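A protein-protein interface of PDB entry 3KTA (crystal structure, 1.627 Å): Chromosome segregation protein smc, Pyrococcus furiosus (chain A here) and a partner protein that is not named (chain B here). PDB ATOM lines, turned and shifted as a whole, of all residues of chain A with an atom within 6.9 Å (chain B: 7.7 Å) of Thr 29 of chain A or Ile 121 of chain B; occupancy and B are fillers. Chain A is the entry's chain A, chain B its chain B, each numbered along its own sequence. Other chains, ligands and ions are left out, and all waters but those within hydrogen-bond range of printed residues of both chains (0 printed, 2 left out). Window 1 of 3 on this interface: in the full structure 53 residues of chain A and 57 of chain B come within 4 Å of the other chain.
The backbone carbonyl oxygen of Phe 28 of chain A sits at hydrogen-bond distance from the backbone NH of Asp 134 of chain B.
The backbone NH of Phe 120 of chain B lies within hydrogen-bond range of the backbone carbonyl oxygen of Gly 27 of chain A (2.8 Å).
The backbone carbonyl oxygen of Thr 29 of chain A sits at hydrogen-bond distance from the backbone NH of Val 122 of chain B, at 2.9 Å.
NE2 of Gln 119 of chain B is in hydrogen-bond range of O of Ser 25 of chain A (2.9 Å).
N of Thr 29 of chain A is in hydrogen-bond range of O of Phe 120 of chain B.
The backbone NH (N) of Ile 4 of chain A sits at hydrogen-bond distance from the side-chain amide oxygen (OE1) of Gln 119 of chain B (2.8 Å).
O of Phe 28 of chain A sits at hydrogen-bond distance from N of Lys 135 of chain B, 3.3 Å away.
The backbone carbonyl oxygen (O) of Val 122 of chain B lies within hydrogen-bond range of the backbone NH (N) of Ile 31 of chain A.
The backbone NH (N) of Ile 137 of chain B lies within hydrogen-bond range of the backbone carbonyl oxygen (O) of Ala 30 of chain A, at 2.8 Å.
N of Ala 30 of chain A is in hydrogen-bond range of O of Lys 135 of chain B, 3.0 Å away.
The backbone carbonyl oxygen (O) of Ile 31 of chain A lies within hydrogen-bond range of the backbone NH (N) of Thr 124 of chain B (3.0 Å).
The side-chain hydroxyl (OG) of Ser 25 of chain A lies within hydrogen-bond range of the backbone NH (N) of Gly 27 of chain A, 2.9 Å away.
O of Ile 123 of chain B is in hydrogen-bond range of N of Glu 94 of chain B (2.8 Å).
N of Ile 121 of chain B lies within hydrogen-bond range of O of Tyr 90 of chain B, at 2.9 Å.
N of Phe 92 of chain B sits at hydrogen-bond distance from O of Ile 121 of chain B, 2.9 Å away.
N of Ser 25 of chain A lies within hydrogen-bond range of OG1 of Thr 29 of chain A (2.9 Å).
CD1 of Ile 137 of chain B touches O of Pro 23 of chain A (3.3 Å).
CD1 of Ile 137 of chain B touches CE1 of Phe 24 of chain A, 3.8 Å away.
OG of Ser 25 of chain A touches CB of Asp 134 of chain B, at 3.5 Å.
Gln 119 of chain B touches Gly 27 of chain A.
O of Phe 120 of chain B touches CA of Phe 28 of chain A (3.4 Å).
CD2 of Phe 28 of chain A touches CA of Ala 133 of chain B (3.6 Å).
Thr 29 of chain A touches Lys 135 of chain B (CA to O, 3.3 Å).
Thr 29 of chain A touches Ile 137 of chain B (CG2 to CD1, 3.7 Å).
Ala 30 of chain A touches Val 122 of chain B.
CA of Ile 136 of chain B touches O of Ala 30 of chain A, at 3.4 Å.
Thr 29 of chain A touches just these residues of chain B: Phe 120 (2.9 Å), Ile 121 (3.6 Å), Val 122 (2.9 Å), Lys 135 (3.3 Å) and Ile 137 (3.7 Å).
Of chain A, only Phe 24, Thr 29 and Ile 31 come within 4 Å of Ile 121 of chain B.
Of the printed residues of chain A, Ile 136 of chain B touches Ala 30 (3.4 Å).
Of the printed residues of chain A, Phe 89 of chain B touches Ile 4 (3.998 Å).
Of the printed residues of chain B, Pro 23 of chain A touches Ile 137.
Printed residues of chain B within 4 Å of Lys 26 of chain A: Gln 119.
Ile 42 of chain A touches none of the printed residues of chain B.
Tyr 90 of chain B touches none of the printed residues of chain A.
The nearest residue of chain B that does not touch Thr 29 of chain A is Ala 133 of chain B (4.6 Å).
The nearest printed residue of chain A that does not touch Phe 120 of chain B is Lys 26 of chain A (4.9 Å).
Of the 24 printed residues of chain B, 13 touch a printed residue of chain A.
Printed residues of chain B that touch a printed residue of chain A: Phe 89, Ile 111, Gln 119, Phe 120, Ile 121, Val 122, Ile 123, Thr 124, Ala 133, Asp 134, Lys 135, Ile 136 and Ile 137.
Of the 13 printed residues of chain A, 10 touch a printed residue of chain B.
Hydrophobic or aromatic side chains of chain A that line the printed part of chain B: Ile 4, Phe 24, Phe 28, Ala 30 and Ile 31.
Along chain A the printed residues that touch a printed residue of chain B span positions 4 to 31.
Among the printed residues, 34 pairs touch across the chains.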
ATOM      1  N   ILE A   4       6.656 -33.280 -10.491  1.00  0.00           N
ATOM      2  CA  ILE A   4       6.376 -33.505  -9.085  1.00  0.00           C
ATOM      3  C   ILE A   4       5.192 -34.454  -8.897  1.00  0.00           C
ATOM      4  O   ILE A   4       4.091 -34.196  -9.376  1.00  0.00           O
ATOM      5  CB  ILE A   4       6.089 -32.177  -8.361  1.00  0.00           C
ATOM      6  CG1 ILE A   4       7.235 -31.186  -8.575  1.00  0.00           C
ATOM      7  CG2 ILE A   4       5.827 -32.428  -6.854  1.00  0.00           C
ATOM      8  CD1 ILE A   4       6.902 -29.760  -8.075  1.00  0.00           C
ATOM      9  N   LEU A   7       4.166 -33.743  -2.565  1.00  0.00           N
ATOM     10  CA  LEU A   7       4.901 -33.221  -1.419  1.00  0.00           C
ATOM     11  C   LEU A   7       4.424 -33.900  -0.139  1.00  0.00           C
ATOM     12  O   LEU A   7       3.259 -34.295  -0.021  1.00  0.00           O
ATOM     13  CB  LEU A   7       4.646 -31.726  -1.235  1.00  0.00           C
ATOM     14  CG  LEU A   7       5.180 -30.771  -2.286  1.00  0.00           C
ATOM     15  CD1 LEU A   7       4.508 -29.420  -2.131  1.00  0.00           C
ATOM     16  CD2 LEU A   7       6.703 -30.632  -2.156  1.00  0.00           C
ATOM     17  N   PRO A  23      -0.707 -34.342  -3.332  1.00  0.00           N
ATOM     18  CA  PRO A  23      -0.428 -34.944  -4.637  1.00  0.00           C
ATOM     19  C   PRO A  23      -0.713 -33.963  -5.758  1.00  0.00           C
ATOM     20  O   PRO A  23      -1.577 -33.098  -5.603  1.00  0.00           O
ATOM     21  CB  PRO A  23      -1.445 -36.084  -4.713  1.00  0.00           C
ATOM     22  CG  PRO A  23      -2.625 -35.551  -3.957  1.00  0.00           C
ATOM     23  CD  PRO A  23      -2.111 -34.551  -2.932  1.00  0.00           C
ATOM     24  N   PHE A  24      -0.006 -34.112  -6.873  1.00  0.00           N
ATOM     25  CA  PHE A  24      -0.202 -33.253  -8.037  1.00  0.00           C
ATOM     26  C   PHE A  24      -0.424 -34.071  -9.305  1.00  0.00           C
ATOM     27  O   PHE A  24       0.114 -35.166  -9.451  1.00  0.00           O
ATOM     28  CB  PHE A  24       1.010 -32.348  -8.252  1.00  0.00           C
ATOM     29  CG  PHE A  24       1.266 -31.428  -7.119  1.00  0.00           C
ATOM     30  CD1 PHE A  24       0.493 -30.290  -6.948  1.00  0.00           C
ATOM     31  CD2 PHE A  24       2.271 -31.695  -6.204  1.00  0.00           C
ATOM     32  CE1 PHE A  24       0.717 -29.425  -5.878  1.00  0.00           C
ATOM     33  CE2 PHE A  24       2.503 -30.832  -5.134  1.00  0.00           C
ATOM     34  CZ  PHE A  24       1.728 -29.701  -4.968  1.00  0.00           C
ATOM     35  N   SER A  25      -1.221 -33.539 -10.227  1.00  0.00           N
ATOM     36  CA  SER A  25      -1.311 -34.124 -11.558  1.00  0.00           C
ATOM     37  C   SER A  25       0.002 -33.894 -12.303  1.00  0.00           C
ATOM     38  O   SER A  25       0.648 -32.879 -12.104  1.00  0.00           O
ATOM     39  CB  SER A  25      -2.445 -33.459 -12.349  1.00  0.00           C
ATOM     40  OG  SER A  25      -2.404 -33.881 -13.703  1.00  0.00           O
ATOM     41  N   LYS A  26       0.389 -34.822 -13.173  1.00  0.00           N
ATOM     42  CA  LYS A  26       1.520 -34.590 -14.075  1.00  0.00           C
ATOM     43  C   LYS A  26       1.274 -33.369 -14.967  1.00  0.00           C
ATOM     44  O   LYS A  26       2.217 -32.731 -15.443  1.00  0.00           O
ATOM     45  CB  LYS A  26       1.749 -35.829 -14.942  1.00  0.00           C
ATOM     46  CG  LYS A  26       2.689 -35.623 -16.096  1.00  0.00           C
ATOM     47  CD  LYS A  26       2.793 -36.900 -16.910  1.00  0.00           C
ATOM     48  CE  LYS A  26       3.691 -36.716 -18.121  1.00  0.00           C
ATOM     49  NZ  LYS A  26       3.896 -38.031 -18.798  1.00  0.00           N
ATOM     50  N   GLY A  27       0.000 -33.040 -15.161  1.00  0.00           N
ATOM     51  CA  GLY A  27      -0.395 -31.923 -15.998  1.00  0.00           C
ATOM     52  C   GLY A  27      -0.687 -30.660 -15.207  1.00  0.00           C
ATOM     53  O   GLY A  27       0.214 -30.049 -14.633  1.00  0.00           O
ATOM     54  N   PHE A  28      -1.965 -30.284 -15.183  1.00  0.00           N
ATOM     55  CA  PHE A  28      -2.427 -29.018 -14.596  1.00  0.00           C
ATOM     56  C   PHE A  28      -3.209 -29.264 -13.298  1.00  0.00           C
ATOM     57  O   PHE A  28      -4.295 -29.857 -13.307  1.00  0.00           O
ATOM     58  CB  PHE A  28      -3.285 -28.320 -15.676  1.00  0.00           C
ATOM     59  CG  PHE A  28      -3.974 -27.048 -15.254  1.00  0.00           C
ATOM     60  CD1 PHE A  28      -3.573 -26.322 -14.145  1.00  0.00           C
ATOM     61  CD2 PHE A  28      -5.028 -26.558 -16.038  1.00  0.00           C
ATOM     62  CE1 PHE A  28      -4.236 -25.141 -13.804  1.00  0.00           C
ATOM     63  CE2 PHE A  28      -5.691 -25.394 -15.710  1.00  0.00           C
ATOM     64  CZ  PHE A  28      -5.296 -24.685 -14.602  1.00  0.00           C
ATOM     65  N   THR A  29      -2.638 -28.843 -12.171  1.00  0.00           N
ATOM     66  CA  THR A  29      -3.338 -28.893 -10.889  1.00  0.00           C
ATOM     67  C   THR A  29      -3.711 -27.478 -10.482  1.00  0.00           C
ATOM     68  O   THR A  29      -2.883 -26.577 -10.539  1.00  0.00           O
ATOM     69  CB  THR A  29      -2.471 -29.505  -9.775  1.00  0.00           C
ATOM     70  OG1 THR A  29      -1.968 -30.780 -10.210  1.00  0.00           O
ATOM     71  CG2 THR A  29      -3.289 -29.676  -8.496  1.00  0.00           C
ATOM     72  N   ALA A  30      -4.963 -27.283 -10.078  1.00  0.00           N
ATOM     73  CA  ALA A  30      -5.374 -26.011  -9.512  1.00  0.00           C
ATOM     74  C   ALA A  30      -5.489 -26.172  -8.008  1.00  0.00           C
ATOM     75  O   ALA A  30      -5.985 -27.193  -7.525  1.00  0.00           O
ATOM     76  CB  ALA A  30      -6.719 -25.567 -10.080  1.00  0.00           C
ATOM     77  N   ILE A  31      -5.051 -25.148  -7.284  1.00  0.00           N
ATOM     78  CA  ILE A  31      -5.149 -25.106  -5.827  1.00  0.00           C
ATOM     79  C   ILE A  31      -6.099 -23.979  -5.458  1.00  0.00           C
ATOM     80  O   ILE A  31      -5.858 -22.823  -5.814  1.00  0.00           O
ATOM     81  CB  ILE A  31      -3.785 -24.849  -5.192  1.00  0.00           C
ATOM     82  CG1 ILE A  31      -2.833 -25.995  -5.546  1.00  0.00           C
ATOM     83  CG2 ILE A  31      -3.920 -24.726  -3.677  1.00  0.00           C
ATOM     84  CD1 ILE A  31      -1.388 -25.736  -5.134  1.00  0.00           C
ATOM     85  N   ILE A  42       2.077 -23.795   0.403  1.00  0.00           N
ATOM     86  CA  ILE A  42       2.453 -24.959  -0.412  1.00  0.00           C
ATOM     87  C   ILE A  42       3.569 -24.602  -1.390  1.00  0.00           C
ATOM     88  O   ILE A  42       4.524 -25.356  -1.560  1.00  0.00           O
ATOM     89  CB  ILE A  42       1.242 -25.532  -1.169  1.00  0.00           C
ATOM     90  CG1 ILE A  42       0.167 -25.981  -0.180  1.00  0.00           C
ATOM     91  CG2 ILE A  42       1.679 -26.664  -2.109  1.00  0.00           C
ATOM     92  CD1 ILE A  42      -1.113 -26.447  -0.864  1.00  0.00           C
ATOM     93  N   ILE A  46       7.753 -25.882  -1.613  1.00  0.00           N
ATOM     94  CA  ILE A  46       8.562 -26.173  -2.793  1.00  0.00           C
ATOM     95  C   ILE A  46       9.863 -25.361  -2.795  1.00  0.00           C
ATOM     96  O   ILE A  46      10.937 -25.917  -3.011  1.00  0.00           O
ATOM     97  CB  ILE A  46       7.763 -25.946  -4.083  1.00  0.00           C
ATOM     98  CG1 ILE A  46       6.568 -26.905  -4.115  1.00  0.00           C
ATOM     99  CG2 ILE A  46       8.682 -26.092  -5.320  1.00  0.00           C
ATOM    100  CD1 ILE A  46       5.575 -26.604  -5.232  1.00  0.00           C
ATOM    101  N   PHE B  89       8.412 -27.956 -14.393  1.00  0.00           N
ATOM    102  CA  PHE B  89       7.141 -27.493 -13.813  1.00  0.00           C
ATOM    103  C   PHE B  89       7.108 -25.981 -13.687  1.00  0.00           C
ATOM    104  O   PHE B  89       8.156 -25.334 -13.669  1.00  0.00           O
ATOM    105  CB  PHE B  89       6.872 -28.139 -12.448  1.00  0.00           C
ATOM    106  CG  PHE B  89       7.779 -27.657 -11.360  1.00  0.00           C
ATOM    107  CD1 PHE B  89       9.005 -28.264 -11.156  1.00  0.00           C
ATOM    108  CD2 PHE B  89       7.410 -26.587 -10.549  1.00  0.00           C
ATOM    109  CE1 PHE B  89       9.834 -27.822 -10.143  1.00  0.00           C
ATOM    110  CE2 PHE B  89       8.234 -26.141  -9.532  1.00  0.00           C
ATOM    111  CZ  PHE B  89       9.462 -26.754  -9.347  1.00  0.00           C
ATOM    112  N   TYR B  90       5.892 -25.438 -13.616  1.00  0.00           N
ATOM    113  CA  TYR B  90       5.666 -24.015 -13.377  1.00  0.00           C
ATOM    114  C   TYR B  90       4.793 -23.918 -12.151  1.00  0.00           C
ATOM    115  O   TYR B  90       3.886 -24.734 -11.976  1.00  0.00           O
ATOM    116  CB  TYR B  90       4.959 -23.356 -14.588  1.00  0.00           C
ATOM    117  CG  TYR B  90       5.875 -23.349 -15.777  1.00  0.00           C
ATOM    118  CD1 TYR B  90       6.045 -24.494 -16.545  1.00  0.00           C
ATOM    119  CD2 TYR B  90       6.625 -22.218 -16.103  1.00  0.00           C
ATOM    120  CE1 TYR B  90       6.939 -24.523 -17.599  1.00  0.00           C
ATOM    121  CE2 TYR B  90       7.515 -22.235 -17.171  1.00  0.00           C
ATOM    122  CZ  TYR B  90       7.663 -23.383 -17.910  1.00  0.00           C
ATOM    123  OH  TYR B  90       8.549 -23.426 -18.952  1.00  0.00           O
ATOM    124  N   LEU B  91       5.083 -22.942 -11.300  1.00  0.00           N
ATOM    125  CA  LEU B  91       4.263 -22.673 -10.124  1.00  0.00           C
ATOM    126  C   LEU B  91       3.786 -21.248 -10.244  1.00  0.00           C
ATOM    127  O   LEU B  91       4.591 -20.325 -10.327  1.00  0.00           O
ATOM    128  CB  LEU B  91       5.079 -22.857  -8.851  1.00  0.00           C
ATOM    129  CG  LEU B  91       4.396 -22.420  -7.558  1.00  0.00           C
ATOM    130  CD1 LEU B  91       3.192 -23.285  -7.236  1.00  0.00           C
ATOM    131  CD2 LEU B  91       5.422 -22.529  -6.447  1.00  0.00           C
ATOM    132  N   PHE B  92       2.471 -21.077 -10.333  1.00  0.00           N
ATOM    133  CA  PHE B  92       1.880 -19.761 -10.537  1.00  0.00           C
ATOM    134  C   PHE B  92       0.943 -19.487  -9.365  1.00  0.00           C
ATOM    135  O   PHE B  92      -0.028 -20.209  -9.171  1.00  0.00           O
ATOM    136  CB  PHE B  92       1.012 -19.743 -11.799  1.00  0.00           C
ATOM    137  CG  PHE B  92       1.760 -19.849 -13.105  1.00  0.00           C
ATOM    138  CD1 PHE B  92       3.100 -19.499 -13.223  1.00  0.00           C
ATOM    139  CD2 PHE B  92       1.071 -20.253 -14.244  1.00  0.00           C
ATOM    140  CE1 PHE B  92       3.751 -19.580 -14.460  1.00  0.00           C
ATOM    141  CE2 PHE B  92       1.701 -20.343 -15.482  1.00  0.00           C
ATOM    142  CZ  PHE B  92       3.044 -20.002 -15.599  1.00  0.00           C
ATOM    143  N   ASP B  93       1.194 -18.420  -8.613  1.00  0.00           N
ATOM    144  CA  ASP B  93       0.346 -18.069  -7.464  1.00  0.00           C
ATOM    145  C   ASP B  93      -0.502 -16.808  -7.726  1.00  0.00           C
ATOM    146  O   ASP B  93       0.008 -15.691  -7.687  1.00  0.00           O
ATOM    147  CB  ASP B  93       1.243 -17.840  -6.250  1.00  0.00           C
ATOM    148  CG  ASP B  93       0.473 -17.794  -4.939  1.00  0.00           C
ATOM    149  OD1 ASP B  93      -0.775 -17.655  -4.960  1.00  0.00           O
ATOM    150  OD2 ASP B  93       1.132 -17.919  -3.887  1.00  0.00           O
ATOM    151  N   GLU B  94      -1.789 -17.009  -8.007  1.00  0.00           N
ATOM    152  CA  GLU B  94      -2.731 -15.922  -8.278  1.00  0.00           C
ATOM    153  C   GLU B  94      -2.229 -14.942  -9.353  1.00  0.00           C
ATOM    154  O   GLU B  94      -2.268 -13.722  -9.191  1.00  0.00           O
ATOM    155  CB  GLU B  94      -3.183 -15.241  -6.978  1.00  0.00           C
ATOM    156  CG  GLU B  94      -3.876 -16.204  -6.046  1.00  0.00           C
ATOM    157  CD  GLU B  94      -4.549 -15.533  -4.873  1.00  0.00           C
ATOM    158  OE1 GLU B  94      -4.394 -16.037  -3.742  1.00  0.00           O
ATOM    159  OE2 GLU B  94      -5.263 -14.509  -5.075  1.00  0.00           O
ATOM    160  N   ILE B  95      -1.807 -15.512 -10.479  1.00  0.00           N
ATOM    161  CA  ILE B  95      -1.262 -14.740 -11.593  1.00  0.00           C
ATOM    162  C   ILE B  95      -2.379 -14.078 -12.376  1.00  0.00           C
ATOM    163  O   ILE B  95      -2.113 -13.260 -13.249  1.00  0.00           O
ATOM    164  CB  ILE B  95      -0.414 -15.599 -12.562  1.00  0.00           C
ATOM    165  CG1 ILE B  95      -1.217 -16.817 -13.058  1.00  0.00           C
ATOM    166  CG2 ILE B  95       0.904 -16.013 -11.899  1.00  0.00           C
ATOM    167  CD1 ILE B  95      -0.905 -17.233 -14.477  1.00  0.00           C
ATOM    168  N   ILE B 111      -2.395 -22.493 -20.669  1.00  0.00           N
ATOM    169  CA  ILE B 111      -1.901 -23.452 -19.676  1.00  0.00           C
ATOM    170  C   ILE B 111      -2.278 -24.889 -20.043  1.00  0.00           C
ATOM    171  O   ILE B 111      -1.420 -25.774 -20.035  1.00  0.00           O
ATOM    172  CB  ILE B 111      -2.374 -23.105 -18.241  1.00  0.00           C
ATOM    173  CG1 ILE B 111      -1.611 -21.890 -17.703  1.00  0.00           C
ATOM    174  CG2 ILE B 111      -2.194 -24.307 -17.294  1.00  0.00           C
ATOM    175  CD1 ILE B 111      -2.322 -21.167 -16.532  1.00  0.00           C
ATOM    176  N   SER B 115       0.393 -27.744 -20.896  1.00  0.00           N
ATOM    177  CA  SER B 115       0.515 -28.833 -19.923  1.00  0.00           C
ATOM    178  C   SER B 115       0.776 -30.184 -20.581  1.00  0.00           C
ATOM    179  O   SER B 115       1.045 -31.163 -19.901  1.00  0.00           O
ATOM    180  CB  SER B 115      -0.720 -28.901 -19.015  1.00  0.00           C
ATOM    181  OG  SER B 115      -1.838 -29.363 -19.748  1.00  0.00           O
ATOM    182  N   SER B 118       4.773 -29.530 -20.014  1.00  0.00           N
ATOM    183  CA  SER B 118       5.256 -29.170 -18.680  1.00  0.00           C
ATOM    184  C   SER B 118       4.144 -29.361 -17.656  1.00  0.00           C
ATOM    185  O   SER B 118       2.962 -29.290 -17.997  1.00  0.00           O
ATOM    186  CB  SER B 118       5.698 -27.696 -18.630  1.00  0.00           C
ATOM    187  OG  SER B 118       6.758 -27.427 -19.530  1.00  0.00           O
ATOM    188  N   GLN B 119       4.527 -29.536 -16.393  1.00  0.00           N
ATOM    189  CA  GLN B 119       3.587 -29.574 -15.287  1.00  0.00           C
ATOM    190  C   GLN B 119       3.271 -28.137 -14.848  1.00  0.00           C
ATOM    191  O   GLN B 119       4.164 -27.287 -14.801  1.00  0.00           O
ATOM    192  CB  GLN B 119       4.217 -30.358 -14.134  1.00  0.00           C
ATOM    193  CG  GLN B 119       3.395 -30.403 -12.853  1.00  0.00           C
ATOM    194  CD  GLN B 119       4.096 -31.273 -11.818  1.00  0.00           C
ATOM    195  OE1 GLN B 119       5.284 -31.076 -11.536  1.00  0.00           O
ATOM    196  NE2 GLN B 119       3.384 -32.248 -11.271  1.00  0.00           N
ATOM    197  N   PHE B 120       2.005 -27.871 -14.538  1.00  0.00           N
ATOM    198  CA  PHE B 120       1.587 -26.569 -14.026  1.00  0.00           C
ATOM    199  C   PHE B 120       0.866 -26.720 -12.708  1.00  0.00           C
ATOM    200  O   PHE B 120      -0.071 -27.528 -12.601  1.00  0.00           O
ATOM    201  CB  PHE B 120       0.657 -25.881 -15.047  1.00  0.00           C
ATOM    202  CG  PHE B 120       1.381 -25.382 -16.241  1.00  0.00           C
ATOM    203  CD1 PHE B 120       1.659 -26.229 -17.315  1.00  0.00           C
ATOM    204  CD2 PHE B 120       1.847 -24.071 -16.286  1.00  0.00           C
ATOM    205  CE1 PHE B 120       2.349 -25.760 -18.417  1.00  0.00           C
ATOM    206  CE2 PHE B 120       2.552 -23.609 -17.376  1.00  0.00           C
ATOM    207  CZ  PHE B 120       2.812 -24.450 -18.439  1.00  0.00           C
ATOM    208  N   ILE B 121       1.291 -25.939 -11.718  1.00  0.00           N
ATOM    209  CA  ILE B 121       0.609 -25.908 -10.425  1.00  0.00           C
ATOM    210  C   ILE B 121       0.170 -24.468 -10.217  1.00  0.00           C
ATOM    211  O   ILE B 121       1.004 -23.558 -10.165  1.00  0.00           O
ATOM    212  CB  ILE B 121       1.554 -26.324  -9.276  1.00  0.00           C
ATOM    213  CG1 ILE B 121       2.021 -27.766  -9.484  1.00  0.00           C
ATOM    214  CG2 ILE B 121       0.859 -26.168  -7.919  1.00  0.00           C
ATOM    215  CD1 ILE B 121       3.277 -28.102  -8.687  1.00  0.00           C
ATOM    216  N   VAL B 122      -1.140 -24.254 -10.128  1.00  0.00           N
ATOM    217  CA  VAL B 122      -1.669 -22.900 -10.188  1.00  0.00           C
ATOM    218  C   VAL B 122      -2.599 -22.653  -9.011  1.00  0.00           C
ATOM    219  O   VAL B 122      -3.590 -23.350  -8.854  1.00  0.00           O
ATOM    220  CB  VAL B 122      -2.479 -22.704 -11.502  1.00  0.00           C
ATOM    221  CG1 VAL B 122      -3.079 -21.296 -11.564  1.00  0.00           C
ATOM    222  CG2 VAL B 122      -1.605 -22.966 -12.731  1.00  0.00           C
ATOM    223  N   ILE B 123      -2.270 -21.661  -8.187  1.00  0.00           N
ATOM    224  CA  ILE B 123      -3.160 -21.239  -7.117  1.00  0.00           C
ATOM    225  C   ILE B 123      -4.072 -20.149  -7.646  1.00  0.00           C
ATOM    226  O   ILE B 123      -3.592 -19.197  -8.261  1.00  0.00           O
ATOM    227  CB  ILE B 123      -2.369 -20.664  -5.950  1.00  0.00           C
ATOM    228  CG1 ILE B 123      -1.466 -21.744  -5.335  1.00  0.00           C
ATOM    229  CG2 ILE B 123      -3.340 -20.090  -4.908  1.00  0.00           C
ATOM    230  CD1 ILE B 123      -0.350 -21.197  -4.443  1.00  0.00           C
ATOM    231  N   THR B 124      -5.378 -20.291  -7.436  1.00  0.00           N
ATOM    232  CA  THR B 124      -6.336 -19.363  -8.059  1.00  0.00           C
ATOM    233  C   THR B 124      -7.666 -19.302  -7.317  1.00  0.00           C
ATOM    234  O   THR B 124      -8.078 -20.276  -6.681  1.00  0.00           O
ATOM    235  CB  THR B 124      -6.593 -19.744  -9.534  1.00  0.00           C
ATOM    236  OG1 THR B 124      -7.490 -18.795 -10.137  1.00  0.00           O
ATOM    237  CG2 THR B 124      -7.198 -21.143  -9.640  1.00  0.00           C
ATOM    238  N   MET B 130      -9.770 -22.344 -13.138  1.00  0.00           N
ATOM    239  CA  MET B 130      -9.860 -23.673 -12.492  1.00  0.00           C
ATOM    240  C   MET B 130     -10.531 -24.754 -13.350  1.00  0.00           C
ATOM    241  O   MET B 130     -10.218 -25.941 -13.231  1.00  0.00           O
ATOM    242  CB  MET B 130     -10.613 -23.550 -11.095  1.00  0.00           C
ATOM    243  CG  MET B 130     -12.183 -24.087 -10.916  1.00  0.00           C
ATOM    244  SD  MET B 130     -12.402 -24.391  -9.016  1.00  0.00           S
ATOM    245  CE  MET B 130     -10.882 -25.579  -8.789  1.00  0.00           C
ATOM    246  N   ASN B 132     -10.953 -26.340 -16.174  1.00  0.00           N
ATOM    247  CA  ASN B 132     -10.409 -27.453 -16.938  1.00  0.00           C
ATOM    248  C   ASN B 132      -9.112 -28.029 -16.384  1.00  0.00           C
ATOM    249  O   ASN B 132      -8.376 -28.688 -17.109  1.00  0.00           O
ATOM    250  CB  ASN B 132     -10.197 -27.039 -18.395  1.00  0.00           C
ATOM    251  CG  ASN B 132     -11.495 -26.729 -19.100  1.00  0.00           C
ATOM    252  OD1 ASN B 132     -12.477 -27.459 -18.960  1.00  0.00           O
ATOM    253  ND2 ASN B 132     -11.512 -25.640 -19.862  1.00  0.00           N
ATOM    254  N   ALA B 133      -8.839 -27.790 -15.105  1.00  0.00           N
ATOM    255  CA  ALA B 133      -7.674 -28.402 -14.467  1.00  0.00           C
ATOM    256  C   ALA B 133      -7.820 -29.924 -14.474  1.00  0.00           C
ATOM    257  O   ALA B 133      -8.938 -30.447 -14.445  1.00  0.00           O
ATOM    258  CB  ALA B 133      -7.538 -27.896 -13.046  1.00  0.00           C
ATOM    259  N   ASP B 134      -6.699 -30.642 -14.524  1.00  0.00           N
ATOM    260  CA  ASP B 134      -6.754 -32.101 -14.475  1.00  0.00           C
ATOM    261  C   ASP B 134      -7.097 -32.597 -13.077  1.00  0.00           C
ATOM    262  O   ASP B 134      -7.788 -33.603 -12.920  1.00  0.00           O
ATOM    263  CB  ASP B 134      -5.420 -32.706 -14.912  1.00  0.00           C
ATOM    264  CG  ASP B 134      -5.067 -32.364 -16.339  1.00  0.00           C
ATOM    265  OD1 ASP B 134      -5.874 -32.673 -17.236  1.00  0.00           O
ATOM    266  OD2 ASP B 134      -3.981 -31.792 -16.572  1.00  0.00           O
ATOM    267  N   LYS B 135      -6.573 -31.903 -12.071  1.00  0.00           N
ATOM    268  CA  LYS B 135      -6.842 -32.190 -10.670  1.00  0.00           C
ATOM    269  C   LYS B 135      -7.035 -30.887  -9.897  1.00  0.00           C
ATOM    270  O   LYS B 135      -6.458 -29.856 -10.250  1.00  0.00           O
ATOM    271  CB  LYS B 135      -5.681 -32.975 -10.044  1.00  0.00           C
ATOM    272  CG  LYS B 135      -5.498 -34.361 -10.636  1.00  0.00           C
ATOM    273  CD  LYS B 135      -6.607 -35.293 -10.126  1.00  0.00           C
ATOM    274  CE  LYS B 135      -6.467 -36.697 -10.697  1.00  0.00           C
ATOM    275  NZ  LYS B 135      -7.479 -37.618 -10.106  1.00  0.00           N
ATOM    276  N   ILE B 136      -7.821 -30.952  -8.826  1.00  0.00           N
ATOM    277  CA  ILE B 136      -8.066 -29.795  -7.980  1.00  0.00           C
ATOM    278  C   ILE B 136      -7.752 -30.149  -6.532  1.00  0.00           C
ATOM    279  O   ILE B 136      -8.211 -31.174  -6.009  1.00  0.00           O
ATOM    280  CB  ILE B 136      -9.549 -29.330  -8.060  1.00  0.00           C
ATOM    281  CG1 ILE B 136      -9.961 -29.126  -9.520  1.00  0.00           C
ATOM    282  CG2 ILE B 136      -9.752 -28.082  -7.231  1.00  0.00           C
ATOM    283  CD1 ILE B 136     -11.482 -29.147  -9.744  1.00  0.00           C
ATOM    284  N   ILE B 137      -6.942 -29.313  -5.899  1.00  0.00           N
ATOM    285  CA  ILE B 137      -6.608 -29.453  -4.491  1.00  0.00           C
ATOM    286  C   ILE B 137      -7.335 -28.361  -3.728  1.00  0.00           C
ATOM    287  O   ILE B 137      -7.268 -27.194  -4.107  1.00  0.00           O
ATOM    288  CB  ILE B 137      -5.089 -29.265  -4.267  1.00  0.00           C
ATOM    289  CG1 ILE B 137      -4.298 -30.398  -4.903  1.00  0.00           C
ATOM    290  CG2 ILE B 137      -4.749 -29.158  -2.783  1.00  0.00           C
ATOM    291  CD1 ILE B 137      -2.824 -30.145  -4.855  1.00  0.00           C
ATOM    292  N   GLY B 138      -8.038 -28.742  -2.663  1.00  0.00           N
ATOM    293  CA  GLY B 138      -8.725 -27.767  -1.836  1.00  0.00           C
ATOM    294  C   GLY B 138      -7.959 -27.530  -0.548  1.00  0.00           C
ATOM    295  O   GLY B 138      -7.569 -28.488   0.121  1.00  0.00           O
